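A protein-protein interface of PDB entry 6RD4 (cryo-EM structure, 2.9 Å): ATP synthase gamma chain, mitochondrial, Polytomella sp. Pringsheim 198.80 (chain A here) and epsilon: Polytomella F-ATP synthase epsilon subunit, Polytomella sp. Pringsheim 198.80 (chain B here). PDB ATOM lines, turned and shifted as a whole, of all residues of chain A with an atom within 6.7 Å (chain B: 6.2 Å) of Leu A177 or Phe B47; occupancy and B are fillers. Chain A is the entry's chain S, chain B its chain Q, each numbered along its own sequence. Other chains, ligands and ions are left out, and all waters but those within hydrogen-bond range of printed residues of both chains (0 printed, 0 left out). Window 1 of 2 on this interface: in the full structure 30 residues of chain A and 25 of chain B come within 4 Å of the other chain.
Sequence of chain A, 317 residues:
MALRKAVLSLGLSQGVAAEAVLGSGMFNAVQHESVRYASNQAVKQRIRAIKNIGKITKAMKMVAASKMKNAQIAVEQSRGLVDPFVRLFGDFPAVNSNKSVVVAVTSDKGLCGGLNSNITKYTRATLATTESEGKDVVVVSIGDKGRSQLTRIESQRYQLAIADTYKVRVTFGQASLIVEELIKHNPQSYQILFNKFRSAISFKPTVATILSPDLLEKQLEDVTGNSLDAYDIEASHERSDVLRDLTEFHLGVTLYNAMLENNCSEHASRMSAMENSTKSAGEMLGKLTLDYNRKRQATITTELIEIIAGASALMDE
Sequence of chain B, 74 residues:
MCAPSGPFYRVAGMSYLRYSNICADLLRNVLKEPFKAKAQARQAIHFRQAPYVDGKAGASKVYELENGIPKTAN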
ATOM      1  N   ILE A 162      -8.606  14.981   0.583  1.00  0.00           N
ATOM      2  CA  ILE A 162      -8.184  16.371   0.464  1.00  0.00           C
ATOM      3  C   ILE A 162      -8.769  17.142   1.637  1.00  0.00           C
ATOM      4  O   ILE A 162      -9.971  17.073   1.900  1.00  0.00           O
ATOM      5  CB  ILE A 162      -8.627  16.990  -0.872  1.00  0.00           C
ATOM      6  CG1 ILE A 162      -7.972  16.305  -2.067  1.00  0.00           C
ATOM      7  CG2 ILE A 162      -8.251  18.442  -0.927  1.00  0.00           C
ATOM      8  CD1 ILE A 162      -8.836  15.313  -2.763  1.00  0.00           C
ATOM      9  N   ALA A 163      -7.918  17.857   2.359  1.00  0.00           N
ATOM     10  CA  ALA A 163      -8.369  18.699   3.444  1.00  0.00           C
ATOM     11  C   ALA A 163      -7.601  20.003   3.372  1.00  0.00           C
ATOM     12  O   ALA A 163      -6.831  20.229   2.439  1.00  0.00           O
ATOM     13  CB  ALA A 163      -8.192  17.998   4.791  1.00  0.00           C
ATOM     14  N   ASP A 164      -7.844  20.865   4.364  1.00  0.00           N
ATOM     15  CA  ASP A 164      -7.229  22.190   4.506  1.00  0.00           C
ATOM     16  C   ASP A 164      -7.509  23.080   3.302  1.00  0.00           C
ATOM     17  O   ASP A 164      -6.714  23.958   2.969  1.00  0.00           O
ATOM     18  CB  ASP A 164      -5.725  22.089   4.765  1.00  0.00           C
ATOM     19  CG  ASP A 164      -5.379  22.147   6.237  1.00  0.00           C
ATOM     20  OD1 ASP A 164      -4.184  21.992   6.570  1.00  0.00           O
ATOM     21  OD2 ASP A 164      -6.299  22.354   7.059  1.00  0.00           O
ATOM     22  N   THR A 165      -8.656  22.870   2.657  1.00  0.00           N
ATOM     23  CA  THR A 165      -8.961  23.536   1.399  1.00  0.00           C
ATOM     24  C   THR A 165      -9.381  24.981   1.610  1.00  0.00           C
ATOM     25  O   THR A 165      -8.832  25.892   0.985  1.00  0.00           O
ATOM     26  CB  THR A 165     -10.066  22.781   0.671  1.00  0.00           C
ATOM     27  OG1 THR A 165      -9.600  21.484   0.293  1.00  0.00           O
ATOM     28  CG2 THR A 165     -10.482  23.511  -0.545  1.00  0.00           C
ATOM     29  N   TYR A 166     -10.332  25.207   2.505  1.00  0.00           N
ATOM     30  CA  TYR A 166     -10.975  26.495   2.662  1.00  0.00           C
ATOM     31  C   TYR A 166     -10.239  27.389   3.642  1.00  0.00           C
ATOM     32  O   TYR A 166     -10.808  28.382   4.101  1.00  0.00           O
ATOM     33  CB  TYR A 166     -12.393  26.298   3.163  1.00  0.00           C
ATOM     34  CG  TYR A 166     -13.143  25.209   2.478  1.00  0.00           C
ATOM     35  CD1 TYR A 166     -13.722  25.399   1.246  1.00  0.00           C
ATOM     36  CD2 TYR A 166     -13.303  23.979   3.093  1.00  0.00           C
ATOM     37  CE1 TYR A 166     -14.419  24.398   0.642  1.00  0.00           C
ATOM     38  CE2 TYR A 166     -14.000  22.973   2.491  1.00  0.00           C
ATOM     39  CZ  TYR A 166     -14.558  23.197   1.266  1.00  0.00           C
ATOM     40  OH  TYR A 166     -15.258  22.206   0.654  1.00  0.00           O
ATOM     41  N   PHE A 172      -8.960  28.355  -8.462  1.00  0.00           N
ATOM     42  CA  PHE A 172      -9.046  27.397  -9.552  1.00  0.00           C
ATOM     43  C   PHE A 172      -7.757  26.621  -9.734  1.00  0.00           C
ATOM     44  O   PHE A 172      -7.800  25.468 -10.167  1.00  0.00           O
ATOM     45  CB  PHE A 172      -9.405  28.092 -10.854  1.00  0.00           C
ATOM     46  CG  PHE A 172      -9.851  27.153 -11.918  1.00  0.00           C
ATOM     47  CD1 PHE A 172      -8.971  26.675 -12.862  1.00  0.00           C
ATOM     48  CD2 PHE A 172     -11.155  26.744 -11.967  1.00  0.00           C
ATOM     49  CE1 PHE A 172      -9.384  25.807 -13.813  1.00  0.00           C
ATOM     50  CE2 PHE A 172     -11.566  25.889 -12.920  1.00  0.00           C
ATOM     51  CZ  PHE A 172     -10.682  25.417 -13.845  1.00  0.00           C
ATOM     52  N   GLY A 173      -6.608  27.230  -9.440  1.00  0.00           N
ATOM     53  CA  GLY A 173      -5.364  26.485  -9.498  1.00  0.00           C
ATOM     54  C   GLY A 173      -5.304  25.406  -8.440  1.00  0.00           C
ATOM     55  O   GLY A 173      -4.743  24.331  -8.662  1.00  0.00           O
ATOM     56  N   GLN A 174      -5.898  25.675  -7.281  1.00  0.00           N
ATOM     57  CA  GLN A 174      -6.034  24.661  -6.247  1.00  0.00           C
ATOM     58  C   GLN A 174      -7.000  23.574  -6.680  1.00  0.00           C
ATOM     59  O   GLN A 174      -6.741  22.386  -6.484  1.00  0.00           O
ATOM     60  CB  GLN A 174      -6.498  25.331  -4.960  1.00  0.00           C
ATOM     61  CG  GLN A 174      -7.006  24.434  -3.885  1.00  0.00           C
ATOM     62  CD  GLN A 174      -7.528  25.241  -2.738  1.00  0.00           C
ATOM     63  OE1 GLN A 174      -7.906  26.396  -2.903  1.00  0.00           O
ATOM     64  NE2 GLN A 174      -7.517  24.662  -1.562  1.00  0.00           N
ATOM     65  N   ALA A 175      -8.112  23.964  -7.299  1.00  0.00           N
ATOM     66  CA  ALA A 175      -9.057  22.977  -7.801  1.00  0.00           C
ATOM     67  C   ALA A 175      -8.537  22.276  -9.043  1.00  0.00           C
ATOM     68  O   ALA A 175      -9.049  21.219  -9.413  1.00  0.00           O
ATOM     69  CB  ALA A 175     -10.388  23.642  -8.095  1.00  0.00           C
ATOM     70  N   SER A 176      -7.543  22.858  -9.716  1.00  0.00           N
ATOM     71  CA  SER A 176      -6.881  22.148 -10.799  1.00  0.00           C
ATOM     72  C   SER A 176      -6.010  21.026 -10.263  1.00  0.00           C
ATOM     73  O   SER A 176      -6.059  19.908 -10.778  1.00  0.00           O
ATOM     74  CB  SER A 176      -6.037  23.110 -11.619  1.00  0.00           C
ATOM     75  OG  SER A 176      -6.838  24.092 -12.236  1.00  0.00           O
ATOM     76  N   LEU A 177      -5.231  21.303  -9.212  1.00  0.00           N
ATOM     77  CA  LEU A 177      -4.331  20.304  -8.642  1.00  0.00           C
ATOM     78  C   LEU A 177      -5.097  19.153  -8.021  1.00  0.00           C
ATOM     79  O   LEU A 177      -4.638  18.010  -8.053  1.00  0.00           O
ATOM     80  CB  LEU A 177      -3.448  20.937  -7.578  1.00  0.00           C
ATOM     81  CG  LEU A 177      -2.385  21.921  -8.006  1.00  0.00           C
ATOM     82  CD1 LEU A 177      -1.591  22.310  -6.795  1.00  0.00           C
ATOM     83  CD2 LEU A 177      -1.497  21.278  -9.039  1.00  0.00           C
ATOM     84  N   ILE A 178      -6.262  19.440  -7.443  1.00  0.00           N
ATOM     85  CA  ILE A 178      -7.124  18.384  -6.926  1.00  0.00           C
ATOM     86  C   ILE A 178      -7.658  17.550  -8.075  1.00  0.00           C
ATOM     87  O   ILE A 178      -7.817  16.331  -7.958  1.00  0.00           O
ATOM     88  CB  ILE A 178      -8.252  19.002  -6.079  1.00  0.00           C
ATOM     89  CG1 ILE A 178      -7.652  19.752  -4.902  1.00  0.00           C
ATOM     90  CG2 ILE A 178      -9.167  17.963  -5.522  1.00  0.00           C
ATOM     91  CD1 ILE A 178      -8.623  20.609  -4.178  1.00  0.00           C
ATOM     92  N   VAL A 179      -7.903  18.187  -9.216  1.00  0.00           N
ATOM     93  CA  VAL A 179      -8.383  17.454 -10.377  1.00  0.00           C
ATOM     94  C   VAL A 179      -7.274  16.632 -11.013  1.00  0.00           C
ATOM     95  O   VAL A 179      -7.524  15.518 -11.465  1.00  0.00           O
ATOM     96  CB  VAL A 179      -9.002  18.410 -11.389  1.00  0.00           C
ATOM     97  N   GLU A 180      -6.033  17.136 -11.020  1.00  0.00           N
ATOM     98  CA  GLU A 180      -4.940  16.369 -11.620  1.00  0.00           C
ATOM     99  C   GLU A 180      -4.582  15.149 -10.784  1.00  0.00           C
ATOM    100  O   GLU A 180      -4.121  14.138 -11.320  1.00  0.00           O
ATOM    101  CB  GLU A 180      -3.703  17.234 -11.833  1.00  0.00           C
ATOM    102  CG  GLU A 180      -3.933  18.439 -12.690  1.00  0.00           C
ATOM    103  CD  GLU A 180      -2.871  19.487 -12.505  1.00  0.00           C
ATOM    104  OE1 GLU A 180      -1.708  19.115 -12.249  1.00  0.00           O
ATOM    105  OE2 GLU A 180      -3.199  20.687 -12.610  1.00  0.00           O
ATOM    106  N   GLU A 181      -4.793  15.221  -9.470  1.00  0.00           N
ATOM    107  CA  GLU A 181      -4.629  14.034  -8.640  1.00  0.00           C
ATOM    108  C   GLU A 181      -5.765  13.046  -8.854  1.00  0.00           C
ATOM    109  O   GLU A 181      -5.633  11.869  -8.512  1.00  0.00           O
ATOM    110  CB  GLU A 181      -4.539  14.427  -7.171  1.00  0.00           C
ATOM    111  CG  GLU A 181      -3.337  15.299  -6.817  1.00  0.00           C
ATOM    112  CD  GLU A 181      -2.004  14.585  -6.921  1.00  0.00           C
ATOM    113  OE1 GLU A 181      -1.948  13.361  -6.673  1.00  0.00           O
ATOM    114  OE2 GLU A 181      -1.001  15.255  -7.240  1.00  0.00           O
ATOM    115  N   LEU A 182      -6.893  13.505  -9.396  1.00  0.00           N
ATOM    116  CA  LEU A 182      -8.003  12.617  -9.711  1.00  0.00           C
ATOM    117  C   LEU A 182      -7.890  11.990 -11.089  1.00  0.00           C
ATOM    118  O   LEU A 182      -8.687  11.110 -11.415  1.00  0.00           O
ATOM    119  CB  LEU A 182      -9.326  13.363  -9.642  1.00  0.00           C
ATOM    120  CG  LEU A 182     -10.231  13.139  -8.445  1.00  0.00           C
ATOM    121  CD1 LEU A 182      -9.549  13.594  -7.190  1.00  0.00           C
ATOM    122  CD2 LEU A 182     -11.477  13.927  -8.683  1.00  0.00           C
ATOM    123  N   LEU A 255     -15.393  21.107 -10.146  1.00  0.00           N
ATOM    124  CA  LEU A 255     -14.830  20.898  -8.824  1.00  0.00           C
ATOM    125  C   LEU A 255     -14.637  22.217  -8.105  1.00  0.00           C
ATOM    126  O   LEU A 255     -14.851  22.305  -6.895  1.00  0.00           O
ATOM    127  CB  LEU A 255     -13.497  20.189  -8.944  1.00  0.00           C
ATOM    128  CG  LEU A 255     -12.992  19.358  -7.793  1.00  0.00           C
ATOM    129  CD1 LEU A 255     -13.934  18.224  -7.546  1.00  0.00           C
ATOM    130  CD2 LEU A 255     -11.641  18.855  -8.172  1.00  0.00           C
ATOM    131  N   LEU B  17      -4.968  21.064 -17.553  1.00  0.00           N
ATOM    132  CA  LEU B  17      -5.284  21.922 -16.417  1.00  0.00           C
ATOM    133  C   LEU B  17      -4.045  22.600 -15.872  1.00  0.00           C
ATOM    134  O   LEU B  17      -4.102  23.760 -15.452  1.00  0.00           O
ATOM    135  CB  LEU B  17      -5.929  21.109 -15.310  1.00  0.00           C
ATOM    136  CG  LEU B  17      -7.352  20.689 -15.558  1.00  0.00           C
ATOM    137  CD1 LEU B  17      -7.622  19.567 -14.613  1.00  0.00           C
ATOM    138  CD2 LEU B  17      -8.256  21.859 -15.297  1.00  0.00           C
ATOM    139  N   ARG B  18      -2.920  21.890 -15.860  1.00  0.00           N
ATOM    140  CA  ARG B  18      -1.693  22.522 -15.414  1.00  0.00           C
ATOM    141  C   ARG B  18      -1.202  23.526 -16.435  1.00  0.00           C
ATOM    142  O   ARG B  18      -0.776  24.620 -16.066  1.00  0.00           O
ATOM    143  CB  ARG B  18      -0.615  21.487 -15.143  1.00  0.00           C
ATOM    144  CG  ARG B  18       0.537  22.079 -14.377  1.00  0.00           C
ATOM    145  CD  ARG B  18       1.544  21.041 -14.017  1.00  0.00           C
ATOM    146  NE  ARG B  18       1.050  20.168 -12.969  1.00  0.00           N
ATOM    147  CZ  ARG B  18       1.338  20.329 -11.690  1.00  0.00           C
ATOM    148  NH1 ARG B  18       2.113  21.334 -11.304  1.00  0.00           N
ATOM    149  NH2 ARG B  18       0.850  19.488 -10.796  1.00  0.00           N
ATOM    150  N   ILE B  45      -2.402  28.694  -3.696  1.00  0.00           N
ATOM    151  CA  ILE B  45      -2.837  27.314  -3.542  1.00  0.00           C
ATOM    152  C   ILE B  45      -2.471  26.869  -2.138  1.00  0.00           C
ATOM    153  O   ILE B  45      -1.286  26.753  -1.809  1.00  0.00           O
ATOM    154  CB  ILE B  45      -2.204  26.387  -4.587  1.00  0.00           C
ATOM    155  CG1 ILE B  45      -2.733  26.721  -5.976  1.00  0.00           C
ATOM    156  CG2 ILE B  45      -2.501  24.945  -4.258  1.00  0.00           C
ATOM    157  CD1 ILE B  45      -2.001  26.022  -7.078  1.00  0.00           C
ATOM    158  N   HIS B  46      -3.485  26.625  -1.311  1.00  0.00           N
ATOM    159  CA  HIS B  46      -3.284  26.184   0.066  1.00  0.00           C
ATOM    160  C   HIS B  46      -4.262  25.046   0.309  1.00  0.00           C
ATOM    161  O   HIS B  46      -5.445  25.294   0.539  1.00  0.00           O
ATOM    162  CB  HIS B  46      -3.516  27.305   1.072  1.00  0.00           C
ATOM    163  CG  HIS B  46      -2.598  28.475   0.923  1.00  0.00           C
ATOM    164  ND1 HIS B  46      -3.013  29.681   0.406  1.00  0.00           N
ATOM    165  CD2 HIS B  46      -1.295  28.631   1.247  1.00  0.00           C
ATOM    166  CE1 HIS B  46      -2.003  30.530   0.413  1.00  0.00           C
ATOM    167  NE2 HIS B  46      -0.948  29.916   0.916  1.00  0.00           N
ATOM    168  N   PHE B  47      -3.772  23.815   0.261  1.00  0.00           N
ATOM    169  CA  PHE B  47      -4.546  22.660   0.689  1.00  0.00           C
ATOM    170  C   PHE B  47      -3.562  21.571   1.085  1.00  0.00           C
ATOM    171  O   PHE B  47      -2.375  21.836   1.286  1.00  0.00           O
ATOM    172  CB  PHE B  47      -5.556  22.216  -0.381  1.00  0.00           C
ATOM    173  CG  PHE B  47      -4.960  21.532  -1.578  1.00  0.00           C
ATOM    174  CD1 PHE B  47      -4.251  22.241  -2.527  1.00  0.00           C
ATOM    175  CD2 PHE B  47      -5.180  20.183  -1.788  1.00  0.00           C
ATOM    176  CE1 PHE B  47      -3.731  21.612  -3.625  1.00  0.00           C
ATOM    177  CE2 PHE B  47      -4.660  19.550  -2.885  1.00  0.00           C
ATOM    178  CZ  PHE B  47      -3.940  20.265  -3.804  1.00  0.00           C
ATOM    179  N   ARG B  48      -4.066  20.358   1.257  1.00  0.00           N
ATOM    180  CA  ARG B  48      -3.229  19.200   1.507  1.00  0.00           C
ATOM    181  C   ARG B  48      -3.988  17.976   1.031  1.00  0.00           C
ATOM    182  O   ARG B  48      -5.209  18.018   0.870  1.00  0.00           O
ATOM    183  CB  ARG B  48      -2.871  19.061   2.987  1.00  0.00           C
ATOM    184  CG  ARG B  48      -4.079  18.799   3.846  1.00  0.00           C
ATOM    185  CD  ARG B  48      -3.742  18.421   5.254  1.00  0.00           C
ATOM    186  NE  ARG B  48      -4.961  17.956   5.895  1.00  0.00           N
ATOM    187  CZ  ARG B  48      -5.025  17.399   7.095  1.00  0.00           C
ATOM    188  NH1 ARG B  48      -6.196  17.006   7.569  1.00  0.00           N
ATOM    189  NH2 ARG B  48      -3.924  17.233   7.812  1.00  0.00           N
ATOM    190  N   GLN B  49      -3.264  16.891   0.783  1.00  0.00           N
ATOM    191  CA  GLN B  49      -3.895  15.655   0.354  1.00  0.00           C
ATOM    192  C   GLN B  49      -3.295  14.492   1.122  1.00  0.00           C
ATOM    193  O   GLN B  49      -2.246  14.615   1.752  1.00  0.00           O
ATOM    194  CB  GLN B  49      -3.746  15.428  -1.155  1.00  0.00           C
ATOM    195  CG  GLN B  49      -2.378  14.973  -1.570  1.00  0.00           C
ATOM    196  CD  GLN B  49      -2.172  15.044  -3.059  1.00  0.00           C
ATOM    197  OE1 GLN B  49      -1.642  16.025  -3.577  1.00  0.00           O
ATOM    198  NE2 GLN B  49      -2.591  14.000  -3.761  1.00  0.00           N
ATOM    199  N   LYS B  61       0.835  15.162   1.195  1.00  0.00           N
ATOM    200  CA  LYS B  61       1.379  16.199   0.330  1.00  0.00           C
ATOM    201  C   LYS B  61       0.690  17.521   0.635  1.00  0.00           C
ATOM    202  O   LYS B  61      -0.440  17.751   0.195  1.00  0.00           O
ATOM    203  CB  LYS B  61       1.179  15.796  -1.125  1.00  0.00           C
ATOM    204  CG  LYS B  61       1.709  16.782  -2.127  1.00  0.00           C
ATOM    205  CD  LYS B  61       3.208  16.764  -2.244  1.00  0.00           C
ATOM    206  CE  LYS B  61       3.630  17.859  -3.186  1.00  0.00           C
ATOM    207  NZ  LYS B  61       2.992  17.678  -4.520  1.00  0.00           N
ATOM    208  N   VAL B  62       1.348  18.386   1.399  1.00  0.00           N
ATOM    209  CA  VAL B  62       0.776  19.671   1.780  1.00  0.00           C
ATOM    210  C   VAL B  62       1.262  20.736   0.811  1.00  0.00           C
ATOM    211  O   VAL B  62       2.296  20.574   0.150  1.00  0.00           O
ATOM    212  CB  VAL B  62       1.109  20.036   3.241  1.00  0.00           C
ATOM    213  CG1 VAL B  62       0.867  18.840   4.151  1.00  0.00           C
ATOM    214  CG2 VAL B  62       2.529  20.562   3.394  1.00  0.00           C
ATOM    215  N   TYR B  63       0.480  21.803   0.677  1.00  0.00           N
ATOM    216  CA  TYR B  63       0.787  22.907  -0.216  1.00  0.00           C
ATOM    217  C   TYR B  63       0.616  24.209   0.546  1.00  0.00           C
ATOM    218  O   TYR B  63      -0.427  24.427   1.168  1.00  0.00           O
ATOM    219  CB  TYR B  63      -0.135  22.893  -1.435  1.00  0.00           C
ATOM    220  CG  TYR B  63      -0.015  21.666  -2.310  1.00  0.00           C
ATOM    221  CD1 TYR B  63      -0.770  20.532  -2.057  1.00  0.00           C
ATOM    222  CD2 TYR B  63       0.834  21.653  -3.403  1.00  0.00           C
ATOM    223  CE1 TYR B  63      -0.668  19.413  -2.851  1.00  0.00           C
ATOM    224  CE2 TYR B  63       0.941  20.539  -4.206  1.00  0.00           C
ATOM    225  CZ  TYR B  63       0.185  19.421  -3.927  1.00  0.00           C
ATOM    226  OH  TYR B  63       0.284  18.301  -4.724  1.00  0.00           O
ATOM    227  N   GLU B  64       1.630  25.066   0.514  1.00  0.00           N
ATOM    228  CA  GLU B  64       1.514  26.438   1.007  1.00  0.00           C
ATOM    229  C   GLU B  64       2.015  27.403  -0.061  1.00  0.00           C
ATOM    230  O   GLU B  64       2.773  28.344   0.181  1.00  0.00           O
ATOM    231  CB  GLU B  64       2.205  26.620   2.369  1.00  0.00           C
ATOM    232  CG  GLU B  64       3.688  26.273   2.456  1.00  0.00           C
ATOM    233  CD  GLU B  64       3.935  24.849   2.908  1.00  0.00           C
ATOM    234  OE1 GLU B  64       2.995  24.027   2.877  1.00  0.00           O
ATOM    235  OE2 GLU B  64       5.079  24.559   3.307  1.00  0.00           O
ATOM    236  N   LEU B  65       1.519  27.177  -1.272  1.00  0.00           N
ATOM    237  CA  LEU B  65       1.964  27.874  -2.470  1.00  0.00           C
ATOM    238  C   LEU B  65       1.295  29.237  -2.559  1.00  0.00           C
ATOM    239  O   LEU B  65       0.095  29.362  -2.304  1.00  0.00           O
ATOM    240  CB  LEU B  65       1.615  27.038  -3.695  1.00  0.00           C
ATOM    241  CG  LEU B  65       2.482  25.893  -4.212  1.00  0.00           C
ATOM    242  CD1 LEU B  65       2.676  24.760  -3.224  1.00  0.00           C
ATOM    243  CD2 LEU B  65       1.801  25.354  -5.427  1.00  0.00           C
ATOM    244  N   ILE B  69       0.564  27.762  -9.473  1.00  0.00           N
ATOM    245  CA  ILE B  69       0.727  26.328  -9.730  1.00  0.00           C
ATOM    246  C   ILE B  69       2.165  26.081 -10.182  1.00  0.00           C
ATOM    247  O   ILE B  69       2.770  26.976 -10.806  1.00  0.00           O
ATOM    248  CB  ILE B  69      -0.320  25.873 -10.775  1.00  0.00           C
ATOM    249  CG1 ILE B  69      -0.513  24.363 -10.847  1.00  0.00           C
ATOM    250  CG2 ILE B  69      -0.048  26.403 -12.171  1.00  0.00           C
ATOM    251  CD1 ILE B  69      -1.711  23.977 -11.666  1.00  0.00           C
ATOM    252  N   PRO B  70       2.803  24.969  -9.798  1.00  0.00           N
ATOM    253  CA  PRO B  70       4.240  24.827 -10.067  1.00  0.00           C
ATOM    254  C   PRO B  70       4.547  24.658 -11.547  1.00  0.00           C
ATOM    255  O   PRO B  70       3.966  23.810 -12.229  1.00  0.00           O
ATOM    256  CB  PRO B  70       4.630  23.579  -9.267  1.00  0.00           C
ATOM    257  CG  PRO B  70       3.642  23.520  -8.192  1.00  0.00           C
ATOM    258  CD  PRO B  70       2.363  23.983  -8.797  1.00  0.00           C
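Among the printed residues, merely in contact across the chains: Gln A174 with Phe B47, Asp A164 with Phe B47, Ile A162 with Arg B48, Leu A177 with Arg B18, Gln A174 with Ile B45, Gly A173 with Ile B45, Ile A178 with Phe B47, Ile A162 with Phe B47, Ala A163 with Phe B47, Val A179 with Leu B17, Leu A177 with Ile B69, Glu A180 with Ile B69, Leu A177 with Ile B45, Asp A164 with Arg B48, Glu A180 with Leu B17 and Leu A177 with Phe B47.
Of the 17 printed residues of chain A, 11 touch a printed residue of chain B.
Printed residues of chain A that touch a printed residue of chain B: Ile A162, Ala A163, Asp A164, Thr A165, Gly A173, Gln A174, Leu A177, Ile A178, Val A179, Glu A180 and Glu A181.
Hydrophobic or aromatic side chains of chain A within 4 Å of the printed part of chain B: Ile A162, Ala A163, Leu A177, Ile A178 and Val A179.
Along chain A the printed residues that touch a printed residue of chain B span positions 162 to 181.
Among the printed residues, 22 pairs touch across the chains.
Of the printed residues of chain B, Asp A164 touches His B46 (3.0 Å), Phe B47 (3.4 Å) and Arg B48 (3.8 Å).
Of the printed residues of chain B, Gln A174 touches Ile B45 (3.6 Å), His B46 (3.0 Å) and Phe B47 (3.4 Å).
Leu A177 touches four residues of chain B.
Of the printed residues of chain B, Glu A181 touches Gln B49 (3.0 Å).
Of chain A, only Ile A162, Ala A163, Asp A164, Gln A174, Leu A177 and Ile A178 come within 4 Å of Phe B47.
Glu B64 touches none of the printed residues of chain A.
The nearest residue of chain B that does not touch Leu A177 is Tyr B63 (4.03 Å).
The guanidinium group (NH1) of Arg B18 lies within hydrogen-bond range of the backbone carbonyl oxygen (O) of Pro B70, at 3.2 Å.
NE2 of His B46 is in hydrogen-bond range of O of Leu B65.
The backbone carbonyl oxygen (O) of Phe B47 is in hydrogen-bond range of the backbone NH (N) of Tyr B63 (2.9 Å).
O of Lys B61 is in hydrogen-bond range of N of Gln B49 (3.0 Å).
The side-chain amide oxygen (OE1) of Gln B49 lies within hydrogen-bond range of the side-chain hydroxyl (OH) of Tyr B63, 3.2 Å away.
The backbone carbonyl oxygen (O) of Thr A165 is in hydrogen-bond range of the side-chain amide nitrogen (NE2) of Gln A174.
The side-chain carboxylate of Glu A180 is in salt-bridge range of the guanidinium group of Arg B18 (3.0 Å).
The backbone carbonyl oxygen of His B46 lies within hydrogen-bond range of the side-chain amide nitrogen of Gln A174 (3.0 Å).
The backbone carbonyl oxygen of Ala A163 is in hydrogen-bond range of the backbone NH of Arg B48 (3.0 Å).
NE2 of Gln B49 is in hydrogen-bond range of OE1 of Glu A181, 3.0 Å away.
The backbone carbonyl oxygen (O) of Asp A164 lies close to the backbone carbonyl oxygen (O) of His B46, at 3.0 Å.
O of Thr A165 lies close to O of His B46 (3.5 Å).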
